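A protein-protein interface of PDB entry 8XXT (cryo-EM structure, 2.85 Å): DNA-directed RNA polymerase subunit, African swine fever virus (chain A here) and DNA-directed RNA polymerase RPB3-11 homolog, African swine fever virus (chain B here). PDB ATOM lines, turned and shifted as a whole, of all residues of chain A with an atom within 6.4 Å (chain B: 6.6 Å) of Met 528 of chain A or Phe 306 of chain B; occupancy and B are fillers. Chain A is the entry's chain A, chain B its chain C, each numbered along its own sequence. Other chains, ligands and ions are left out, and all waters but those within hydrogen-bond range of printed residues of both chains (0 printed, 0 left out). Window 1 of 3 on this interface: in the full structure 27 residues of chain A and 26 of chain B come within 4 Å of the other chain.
O of Ile 304 of chain B sits at hydrogen-bond distance from NZ of Lys 524 of chain A, at 2.7 Å.
N of Leu 525 of chain A lies within hydrogen-bond range of OH of Tyr 298 of chain B (3.5 Å).
The side-chain sulfur of Met 528 of chain A is in hydrogen-bond range of the backbone NH of Val 307 of chain B (3.5 Å).
The side-chain amino group (NZ) of Lys 294 of chain B sits close to the side-chain amide nitrogen (NE2) of Gln 532 of chain A (3.0 Å).
SG of Cys 540 of chain A lies within hydrogen-bond range of OG of Ser 305 of chain B (3.2 Å).
The backbone carbonyl oxygen of Ser 305 of chain B sits at hydrogen-bond distance from the backbone NH of Phe 541 of chain A.
OD1 of Asn 523 of chain A lies within hydrogen-bond range of N of Leu 525 of chain A (2.7 Å).
The side-chain amide nitrogen (ND2) of Asn 523 of chain A lies within hydrogen-bond range of a ring nitrogen (ND1) of His 526 of chain A (3.0 Å).
The backbone carbonyl oxygen (O) of Phe 541 of chain A lies within hydrogen-bond range of the side-chain amino group (NZ) of Lys 524 of chain A (3.2 Å).
The backbone carbonyl oxygen (O) of Ile 323 of chain B lies within hydrogen-bond range of the backbone NH (N) of Ser 305 of chain B.
The backbone carbonyl oxygen of Phe 306 of chain B sits at hydrogen-bond distance from the backbone NH of Ile 323 of chain B.
The backbone carbonyl oxygen of Gly 308 of chain B lies within hydrogen-bond range of the backbone NH of Thr 321 of chain B, 2.7 Å away.
Among the printed residues, merely in contact across the chains: Gln 532 of chain A with Tyr 309 of chain B, Pro 538 of chain A with Phe 306 of chain B, Lys 524 of chain A with Asp 303 of chain B, Met 528 of chain A with Phe 306 of chain B, Lys 524 of chain A with Tyr 298 of chain B, Met 528 of chain A with Tyr 298 of chain B, Pro 538 of chain A with Ile 323 of chain B, Phe 541 of chain A with Ile 304 of chain B, Pro 539 of chain A with Ser 305 of chain B, Asn 523 of chain A with Tyr 298 of chain B, Ala 542 of chain A with Ile 304 of chain B, Ala 542 of chain A with Asp 303 of chain B, Gln 532 of chain A with Gly 308 of chain B and Ala 542 of chain A with Ser 305 of chain B.
Printed residues of chain B within 4 Å of Met 528 of chain A: Tyr 298 (3.6 Å), Phe 306 (3.5 Å) and Val 307 (3.5 Å).
Printed residues of chain A within 4 Å of Phe 306 of chain B: Met 528 and Pro 538.
Printed residues of chain A within 4 Å of Tyr 298 of chain B: Asn 523, Lys 524, Leu 525 and Met 528.
Printed residues of chain A within 4 Å of Asp 303 of chain B: Lys 524 and Ala 542.
Printed residues of chain A within 4 Å of Val 307 of chain B: Met 528 (3.5 Å).
Of the printed residues of chain B, Gln 532 of chain A touches Lys 294 (3.0 Å), Gly 308 (3.9 Å) and Tyr 309 (3.4 Å).
Ile 322 of chain B touches none of the printed residues of chain A.
Leu 530 of chain A touches none of the printed residues of chain B.
Hydrophobic or aromatic side chains of chain A that line the printed part of chain B: Leu 525, Met 528, Pro 538 and Phe 541.
Among the printed residues, 20 pairs touch across the chains.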
ATOM      1  N   ASN A 523     -33.588   6.958  12.159  1.00  0.00           N
ATOM      2  CA  ASN A 523     -32.916   8.199  11.825  1.00  0.00           C
ATOM      3  C   ASN A 523     -31.433   7.934  11.580  1.00  0.00           C
ATOM      4  O   ASN A 523     -30.951   6.802  11.656  1.00  0.00           O
ATOM      5  CB  ASN A 523     -33.143   9.237  12.920  1.00  0.00           C
ATOM      6  CG  ASN A 523     -32.364   8.941  14.178  1.00  0.00           C
ATOM      7  OD1 ASN A 523     -31.177   9.236  14.271  1.00  0.00           O
ATOM      8  ND2 ASN A 523     -33.036   8.374  15.167  1.00  0.00           N
ATOM      9  N   LYS A 524     -30.701   9.003  11.266  1.00  0.00           N
ATOM     10  CA  LYS A 524     -29.302   8.858  10.876  1.00  0.00           C
ATOM     11  C   LYS A 524     -28.458   8.295  12.012  1.00  0.00           C
ATOM     12  O   LYS A 524     -27.579   7.458  11.781  1.00  0.00           O
ATOM     13  CB  LYS A 524     -28.754  10.206  10.415  1.00  0.00           C
ATOM     14  CG  LYS A 524     -27.280  10.203  10.070  1.00  0.00           C
ATOM     15  CD  LYS A 524     -26.818  11.601   9.724  1.00  0.00           C
ATOM     16  CE  LYS A 524     -25.343  11.640   9.423  1.00  0.00           C
ATOM     17  NZ  LYS A 524     -24.949  12.944   8.835  1.00  0.00           N
ATOM     18  N   LEU A 525     -28.706   8.742  13.244  1.00  0.00           N
ATOM     19  CA  LEU A 525     -27.879   8.316  14.369  1.00  0.00           C
ATOM     20  C   LEU A 525     -27.985   6.817  14.607  1.00  0.00           C
ATOM     21  O   LEU A 525     -26.988   6.159  14.917  1.00  0.00           O
ATOM     22  CB  LEU A 525     -28.272   9.081  15.628  1.00  0.00           C
ATOM     23  CG  LEU A 525     -27.423   8.796  16.863  1.00  0.00           C
ATOM     24  CD1 LEU A 525     -25.997   9.257  16.645  1.00  0.00           C
ATOM     25  CD2 LEU A 525     -28.023   9.464  18.080  1.00  0.00           C
ATOM     26  N   HIS A 526     -29.187   6.262  14.490  1.00  0.00           N
ATOM     27  CA  HIS A 526     -29.378   4.835  14.695  1.00  0.00           C
ATOM     28  C   HIS A 526     -29.028   4.003  13.474  1.00  0.00           C
ATOM     29  O   HIS A 526     -28.695   2.824  13.623  1.00  0.00           O
ATOM     30  CB  HIS A 526     -30.818   4.556  15.122  1.00  0.00           C
ATOM     31  CG  HIS A 526     -31.136   5.058  16.492  1.00  0.00           C
ATOM     32  ND1 HIS A 526     -31.554   6.347  16.732  1.00  0.00           N
ATOM     33  CD2 HIS A 526     -31.068   4.453  17.699  1.00  0.00           C
ATOM     34  CE1 HIS A 526     -31.745   6.512  18.029  1.00  0.00           C
ATOM     35  NE2 HIS A 526     -31.458   5.377  18.638  1.00  0.00           N
ATOM     36  N   ALA A 527     -29.099   4.577  12.274  1.00  0.00           N
ATOM     37  CA  ALA A 527     -28.548   3.892  11.113  1.00  0.00           C
ATOM     38  C   ALA A 527     -27.033   3.802  11.208  1.00  0.00           C
ATOM     39  O   ALA A 527     -26.443   2.779  10.847  1.00  0.00           O
ATOM     40  CB  ALA A 527     -28.969   4.602   9.830  1.00  0.00           C
ATOM     41  N   MET A 528     -26.388   4.865  11.691  1.00  0.00           N
ATOM     42  CA  MET A 528     -24.948   4.823  11.923  1.00  0.00           C
ATOM     43  C   MET A 528     -24.595   3.800  12.993  1.00  0.00           C
ATOM     44  O   MET A 528     -23.582   3.102  12.883  1.00  0.00           O
ATOM     45  CB  MET A 528     -24.435   6.203  12.330  1.00  0.00           C
ATOM     46  CG  MET A 528     -24.343   7.197  11.200  1.00  0.00           C
ATOM     47  SD  MET A 528     -23.391   8.655  11.648  1.00  0.00           S
ATOM     48  CE  MET A 528     -24.310   9.214  13.072  1.00  0.00           C
ATOM     49  N   GLY A 529     -25.414   3.705  14.039  1.00  0.00           N
ATOM     50  CA  GLY A 529     -25.119   2.782  15.119  1.00  0.00           C
ATOM     51  C   GLY A 529     -25.170   1.327  14.703  1.00  0.00           C
ATOM     52  O   GLY A 529     -24.590   0.468  15.367  1.00  0.00           O
ATOM     53  N   LEU A 530     -25.867   1.025  13.607  1.00  0.00           N
ATOM     54  CA  LEU A 530     -25.900  -0.350  13.124  1.00  0.00           C
ATOM     55  C   LEU A 530     -24.540  -0.791  12.610  1.00  0.00           C
ATOM     56  O   LEU A 530     -24.263  -1.993  12.541  1.00  0.00           O
ATOM     57  CB  LEU A 530     -26.948  -0.509  12.024  1.00  0.00           C
ATOM     58  CG  LEU A 530     -28.418  -0.336  12.400  1.00  0.00           C
ATOM     59  CD1 LEU A 530     -29.299  -1.023  11.383  1.00  0.00           C
ATOM     60  CD2 LEU A 530     -28.682  -0.881  13.781  1.00  0.00           C
ATOM     61  N   PHE A 531     -23.683   0.158  12.242  1.00  0.00           N
ATOM     62  CA  PHE A 531     -22.386  -0.142  11.658  1.00  0.00           C
ATOM     63  C   PHE A 531     -21.239   0.036  12.642  1.00  0.00           C
ATOM     64  O   PHE A 531     -20.076  -0.019  12.236  1.00  0.00           O
ATOM     65  CB  PHE A 531     -22.157   0.735  10.427  1.00  0.00           C
ATOM     66  CG  PHE A 531     -23.033   0.383   9.265  1.00  0.00           C
ATOM     67  CD1 PHE A 531     -22.638  -0.568   8.346  1.00  0.00           C
ATOM     68  CD2 PHE A 531     -24.256   1.003   9.094  1.00  0.00           C
ATOM     69  CE1 PHE A 531     -23.447  -0.891   7.278  1.00  0.00           C
ATOM     70  CE2 PHE A 531     -25.066   0.680   8.030  1.00  0.00           C
ATOM     71  CZ  PHE A 531     -24.661  -0.267   7.122  1.00  0.00           C
ATOM     72  N   GLN A 532     -21.538   0.255  13.921  1.00  0.00           N
ATOM     73  CA  GLN A 532     -20.482   0.476  14.901  1.00  0.00           C
ATOM     74  C   GLN A 532     -19.607  -0.759  15.060  1.00  0.00           C
ATOM     75  O   GLN A 532     -18.376  -0.662  15.104  1.00  0.00           O
ATOM     76  CB  GLN A 532     -21.089   0.859  16.247  1.00  0.00           C
ATOM     77  CG  GLN A 532     -21.688   2.235  16.304  1.00  0.00           C
ATOM     78  CD  GLN A 532     -22.547   2.413  17.525  1.00  0.00           C
ATOM     79  OE1 GLN A 532     -22.958   1.440  18.151  1.00  0.00           O
ATOM     80  NE2 GLN A 532     -22.820   3.658  17.882  1.00  0.00           N
ATOM     81  N   PRO A 538     -16.889   1.993   7.835  1.00  0.00           N
ATOM     82  CA  PRO A 538     -18.291   2.388   7.848  1.00  0.00           C
ATOM     83  C   PRO A 538     -18.659   3.135   6.580  1.00  0.00           C
ATOM     84  O   PRO A 538     -17.818   3.830   5.985  1.00  0.00           O
ATOM     85  CB  PRO A 538     -18.388   3.300   9.083  1.00  0.00           C
ATOM     86  CG  PRO A 538     -17.012   3.807   9.265  1.00  0.00           C
ATOM     87  CD  PRO A 538     -16.102   2.703   8.854  1.00  0.00           C
ATOM     88  N   PRO A 539     -19.902   3.023   6.130  1.00  0.00           N
ATOM     89  CA  PRO A 539     -20.320   3.755   4.928  1.00  0.00           C
ATOM     90  C   PRO A 539     -20.411   5.252   5.164  1.00  0.00           C
ATOM     91  O   PRO A 539     -20.057   5.742   6.240  1.00  0.00           O
ATOM     92  CB  PRO A 539     -21.689   3.145   4.610  1.00  0.00           C
ATOM     93  CG  PRO A 539     -22.167   2.602   5.901  1.00  0.00           C
ATOM     94  CD  PRO A 539     -20.958   2.135   6.635  1.00  0.00           C
ATOM     95  N   CYS A 540     -20.872   5.991   4.162  1.00  0.00           N
ATOM     96  CA  CYS A 540     -20.951   7.442   4.235  1.00  0.00           C
ATOM     97  C   CYS A 540     -22.392   7.865   4.474  1.00  0.00           C
ATOM     98  O   CYS A 540     -23.295   7.468   3.731  1.00  0.00           O
ATOM     99  CB  CYS A 540     -20.415   8.079   2.953  1.00  0.00           C
ATOM    100  SG  CYS A 540     -20.044   9.840   3.087  1.00  0.00           S
ATOM    101  N   PHE A 541     -22.601   8.668   5.514  1.00  0.00           N
ATOM    102  CA  PHE A 541     -23.916   9.194   5.849  1.00  0.00           C
ATOM    103  C   PHE A 541     -24.014  10.694   5.620  1.00  0.00           C
ATOM    104  O   PHE A 541     -24.949  11.325   6.120  1.00  0.00           O
ATOM    105  CB  PHE A 541     -24.259   8.871   7.302  1.00  0.00           C
ATOM    106  CG  PHE A 541     -24.457   7.413   7.567  1.00  0.00           C
ATOM    107  CD1 PHE A 541     -25.707   6.838   7.446  1.00  0.00           C
ATOM    108  CD2 PHE A 541     -23.392   6.616   7.943  1.00  0.00           C
ATOM    109  CE1 PHE A 541     -25.888   5.499   7.691  1.00  0.00           C
ATOM    110  CE2 PHE A 541     -23.571   5.277   8.190  1.00  0.00           C
ATOM    111  CZ  PHE A 541     -24.818   4.717   8.064  1.00  0.00           C
ATOM    112  N   ALA A 542     -23.070  11.281   4.880  1.00  0.00           N
ATOM    113  CA  ALA A 542     -23.057  12.729   4.710  1.00  0.00           C
ATOM    114  C   ALA A 542     -24.277  13.223   3.948  1.00  0.00           C
ATOM    115  O   ALA A 542     -24.669  14.385   4.091  1.00  0.00           O
ATOM    116  CB  ALA A 542     -21.778  13.158   3.995  1.00  0.00           C
ATOM    117  N   LEU A 550     -33.970   6.403   7.388  1.00  0.00           N
ATOM    118  CA  LEU A 550     -33.362   5.386   6.546  1.00  0.00           C
ATOM    119  C   LEU A 550     -34.135   4.084   6.692  1.00  0.00           C
ATOM    120  O   LEU A 550     -34.345   3.605   7.810  1.00  0.00           O
ATOM    121  CB  LEU A 550     -31.896   5.171   6.922  1.00  0.00           C
ATOM    122  CG  LEU A 550     -30.914   6.305   6.629  1.00  0.00           C
ATOM    123  CD1 LEU A 550     -30.843   7.269   7.792  1.00  0.00           C
ATOM    124  CD2 LEU A 550     -29.541   5.743   6.328  1.00  0.00           C
ATOM    125  N   VAL A 555     -29.972   0.229   4.798  1.00  0.00           N
ATOM    126  CA  VAL A 555     -28.696   0.004   5.469  1.00  0.00           C
ATOM    127  C   VAL A 555     -28.093  -1.332   5.058  1.00  0.00           C
ATOM    128  O   VAL A 555     -26.868  -1.470   4.966  1.00  0.00           O
ATOM    129  CB  VAL A 555     -28.866   0.103   6.995  1.00  0.00           C
ATOM    130  CG1 VAL A 555     -29.227   1.518   7.389  1.00  0.00           C
ATOM    131  CG2 VAL A 555     -29.919  -0.865   7.475  1.00  0.00           C
ATOM    132  N   LYS B 294     -20.380  10.263  21.196  1.00  0.00           N
ATOM    133  CA  LYS B 294     -21.095  10.057  19.942  1.00  0.00           C
ATOM    134  C   LYS B 294     -22.266  11.019  19.817  1.00  0.00           C
ATOM    135  O   LYS B 294     -22.416  11.703  18.799  1.00  0.00           O
ATOM    136  CB  LYS B 294     -21.575   8.611  19.843  1.00  0.00           C
ATOM    137  CG  LYS B 294     -22.222   8.273  18.517  1.00  0.00           C
ATOM    138  CD  LYS B 294     -22.792   6.873  18.519  1.00  0.00           C
ATOM    139  CE  LYS B 294     -24.020   6.781  19.396  1.00  0.00           C
ATOM    140  NZ  LYS B 294     -24.846   5.589  19.071  1.00  0.00           N
ATOM    141  N   ILE B 297     -20.990  14.805  19.515  1.00  0.00           N
ATOM    142  CA  ILE B 297     -20.354  15.032  18.223  1.00  0.00           C
ATOM    143  C   ILE B 297     -21.404  15.067  17.125  1.00  0.00           C
ATOM    144  O   ILE B 297     -21.365  15.918  16.231  1.00  0.00           O
ATOM    145  CB  ILE B 297     -19.288  13.954  17.960  1.00  0.00           C
ATOM    146  CG1 ILE B 297     -18.052  14.212  18.820  1.00  0.00           C
ATOM    147  CG2 ILE B 297     -18.913  13.915  16.496  1.00  0.00           C
ATOM    148  CD1 ILE B 297     -17.169  13.005  18.993  1.00  0.00           C
ATOM    149  N   TYR B 298     -22.369  14.151  17.188  1.00  0.00           N
ATOM    150  CA  TYR B 298     -23.448  14.126  16.211  1.00  0.00           C
ATOM    151  C   TYR B 298     -24.317  15.373  16.295  1.00  0.00           C
ATOM    152  O   TYR B 298     -24.787  15.870  15.267  1.00  0.00           O
ATOM    153  CB  TYR B 298     -24.267  12.862  16.435  1.00  0.00           C
ATOM    154  CG  TYR B 298     -25.494  12.707  15.587  1.00  0.00           C
ATOM    155  CD1 TYR B 298     -25.397  12.477  14.225  1.00  0.00           C
ATOM    156  CD2 TYR B 298     -26.752  12.746  16.158  1.00  0.00           C
ATOM    157  CE1 TYR B 298     -26.521  12.315  13.457  1.00  0.00           C
ATOM    158  CE2 TYR B 298     -27.876  12.586  15.400  1.00  0.00           C
ATOM    159  CZ  TYR B 298     -27.757  12.369  14.052  1.00  0.00           C
ATOM    160  OH  TYR B 298     -28.892  12.202  13.305  1.00  0.00           O
ATOM    161  N   ASP B 303     -24.147  16.944   9.820  1.00  0.00           N
ATOM    162  CA  ASP B 303     -23.832  16.444   8.489  1.00  0.00           C
ATOM    163  C   ASP B 303     -22.645  15.492   8.481  1.00  0.00           C
ATOM    164  O   ASP B 303     -22.015  15.313   7.434  1.00  0.00           O
ATOM    165  CB  ASP B 303     -23.560  17.613   7.542  1.00  0.00           C
ATOM    166  CG  ASP B 303     -22.598  18.627   8.132  1.00  0.00           C
ATOM    167  OD1 ASP B 303     -22.395  18.611   9.363  1.00  0.00           O
ATOM    168  OD2 ASP B 303     -22.044  19.440   7.364  1.00  0.00           O
ATOM    169  N   ILE B 304     -22.332  14.876   9.624  1.00  0.00           N
ATOM    170  CA  ILE B 304     -21.138  14.053   9.726  1.00  0.00           C
ATOM    171  C   ILE B 304     -21.249  12.833   8.816  1.00  0.00           C
ATOM    172  O   ILE B 304     -22.342  12.321   8.545  1.00  0.00           O
ATOM    173  CB  ILE B 304     -20.902  13.639  11.189  1.00  0.00           C
ATOM    174  CG1 ILE B 304     -19.467  13.167  11.395  1.00  0.00           C
ATOM    175  CG2 ILE B 304     -21.889  12.574  11.617  1.00  0.00           C
ATOM    176  CD1 ILE B 304     -19.035  13.200  12.828  1.00  0.00           C
ATOM    177  N   SER B 305     -20.099  12.381   8.313  1.00  0.00           N
ATOM    178  CA  SER B 305     -20.078  11.192   7.469  1.00  0.00           C
ATOM    179  C   SER B 305     -20.314   9.931   8.288  1.00  0.00           C
ATOM    180  O   SER B 305     -21.068   9.048   7.870  1.00  0.00           O
ATOM    181  CB  SER B 305     -18.752  11.105   6.720  1.00  0.00           C
ATOM    182  OG  SER B 305     -18.660   9.896   5.993  1.00  0.00           O
ATOM    183  N   PHE B 306     -19.674   9.830   9.451  1.00  0.00           N
ATOM    184  CA  PHE B 306     -19.888   8.712  10.360  1.00  0.00           C
ATOM    185  C   PHE B 306     -19.297   9.012  11.727  1.00  0.00           C
ATOM    186  O   PHE B 306     -18.140   9.427  11.829  1.00  0.00           O
ATOM    187  CB  PHE B 306     -19.270   7.424   9.813  1.00  0.00           C
ATOM    188  CG  PHE B 306     -19.363   6.259  10.760  1.00  0.00           C
ATOM    189  CD1 PHE B 306     -20.498   5.469  10.794  1.00  0.00           C
ATOM    190  CD2 PHE B 306     -18.323   5.958  11.620  1.00  0.00           C
ATOM    191  CE1 PHE B 306     -20.589   4.404  11.662  1.00  0.00           C
ATOM    192  CE2 PHE B 306     -18.411   4.894  12.489  1.00  0.00           C
ATOM    193  CZ  PHE B 306     -19.546   4.116  12.509  1.00  0.00           C
ATOM    194  N   VAL B 307     -20.079   8.809  12.782  1.00  0.00           N
ATOM    195  CA  VAL B 307     -19.571   8.795  14.146  1.00  0.00           C
ATOM    196  C   VAL B 307     -20.118   7.554  14.831  1.00  0.00           C
ATOM    197  O   VAL B 307     -21.303   7.235  14.695  1.00  0.00           O
ATOM    198  CB  VAL B 307     -19.938  10.071  14.927  1.00  0.00           C
ATOM    199  CG1 VAL B 307     -21.437  10.265  14.990  1.00  0.00           C
ATOM    200  CG2 VAL B 307     -19.343  10.020  16.319  1.00  0.00           C
ATOM    201  N   GLY B 308     -19.251   6.836  15.527  1.00  0.00           N
ATOM    202  CA  GLY B 308     -19.663   5.620  16.197  1.00  0.00           C
ATOM    203  C   GLY B 308     -18.632   5.210  17.216  1.00  0.00           C
ATOM    204  O   GLY B 308     -17.449   5.536  17.095  1.00  0.00           O
ATOM    205  N   TYR B 309     -19.088   4.492  18.230  1.00  0.00           N
ATOM    206  CA  TYR B 309     -18.226   3.981  19.277  1.00  0.00           C
ATOM    207  C   TYR B 309     -18.570   2.526  19.527  1.00  0.00           C
ATOM    208  O   TYR B 309     -19.685   2.081  19.247  1.00  0.00           O
ATOM    209  CB  TYR B 309     -18.379   4.782  20.572  1.00  0.00           C
ATOM    210  CG  TYR B 309     -19.487   4.272  21.457  1.00  0.00           C
ATOM    211  CD1 TYR B 309     -20.817   4.473  21.121  1.00  0.00           C
ATOM    212  CD2 TYR B 309     -19.207   3.580  22.625  1.00  0.00           C
ATOM    213  CE1 TYR B 309     -21.829   4.003  21.918  1.00  0.00           C
ATOM    214  CE2 TYR B 309     -20.216   3.106  23.429  1.00  0.00           C
ATOM    215  CZ  TYR B 309     -21.525   3.321  23.071  1.00  0.00           C
ATOM    216  OH  TYR B 309     -22.536   2.852  23.870  1.00  0.00           O
ATOM    217  N   THR B 321     -14.878   6.169  16.582  1.00  0.00           N
ATOM    218  CA  THR B 321     -14.476   6.445  15.212  1.00  0.00           C
ATOM    219  C   THR B 321     -15.286   7.612  14.673  1.00  0.00           C
ATOM    220  O   THR B 321     -16.519   7.596  14.730  1.00  0.00           O
ATOM    221  CB  THR B 321     -14.674   5.216  14.323  1.00  0.00           C
ATOM    222  OG1 THR B 321     -13.844   4.147  14.791  1.00  0.00           O
ATOM    223  CG2 THR B 321     -14.316   5.533  12.883  1.00  0.00           C
ATOM    224  N   ILE B 322     -14.593   8.620  14.153  1.00  0.00           N
ATOM    225  CA  ILE B 322     -15.219   9.777  13.526  1.00  0.00           C
ATOM    226  C   ILE B 322     -14.681   9.903  12.110  1.00  0.00           C
ATOM    227  O   ILE B 322     -13.465   9.875  11.897  1.00  0.00           O
ATOM    228  CB  ILE B 322     -14.962  11.071  14.317  1.00  0.00           C
ATOM    229  CG1 ILE B 322     -15.431  10.922  15.759  1.00  0.00           C
ATOM    230  CG2 ILE B 322     -15.665  12.235  13.664  1.00  0.00           C
ATOM    231  CD1 ILE B 322     -14.313  10.943  16.758  1.00  0.00           C
ATOM    232  N   ILE B 323     -15.586  10.033  11.146  1.00  0.00           N
ATOM    233  CA  ILE B 323     -15.240  10.311   9.761  1.00  0.00           C
ATOM    234  C   ILE B 323     -16.037  11.531   9.328  1.00  0.00           C
ATOM    235  O   ILE B 323     -17.255  11.576   9.519  1.00  0.00           O
ATOM    236  CB  ILE B 323     -15.539   9.113   8.843  1.00  0.00           C
ATOM    237  CG1 ILE B 323     -14.810   7.870   9.340  1.00  0.00           C
ATOM    238  CG2 ILE B 323     -15.136   9.422   7.417  1.00  0.00           C
ATOM    239  CD1 ILE B 323     -14.964   6.685   8.428  1.00  0.00           C
ATOM    240  N   HIS B 324     -15.355  12.519   8.755  1.00  0.00           N
ATOM    241  CA  HIS B 324     -16.002  13.781   8.436  1.00  0.00           C
ATOM    242  C   HIS B 324     -15.338  14.405   7.220  1.00  0.00           C
ATOM    243  O   HIS B 324     -14.137  14.236   6.998  1.00  0.00           O
ATOM    244  CB  HIS B 324     -15.940  14.741   9.627  1.00  0.00           C
ATOM    245  CG  HIS B 324     -16.698  16.013   9.422  1.00  0.00           C
ATOM    246  ND1 HIS B 324     -17.862  16.077   8.690  1.00  0.00           N
ATOM    247  CD2 HIS B 324     -16.460  17.272   9.860  1.00  0.00           C
ATOM    248  CE1 HIS B 324     -18.307  17.320   8.682  1.00  0.00           C
ATOM    249  NE2 HIS B 324     -17.474  18.065   9.385  1.00  0.00           N
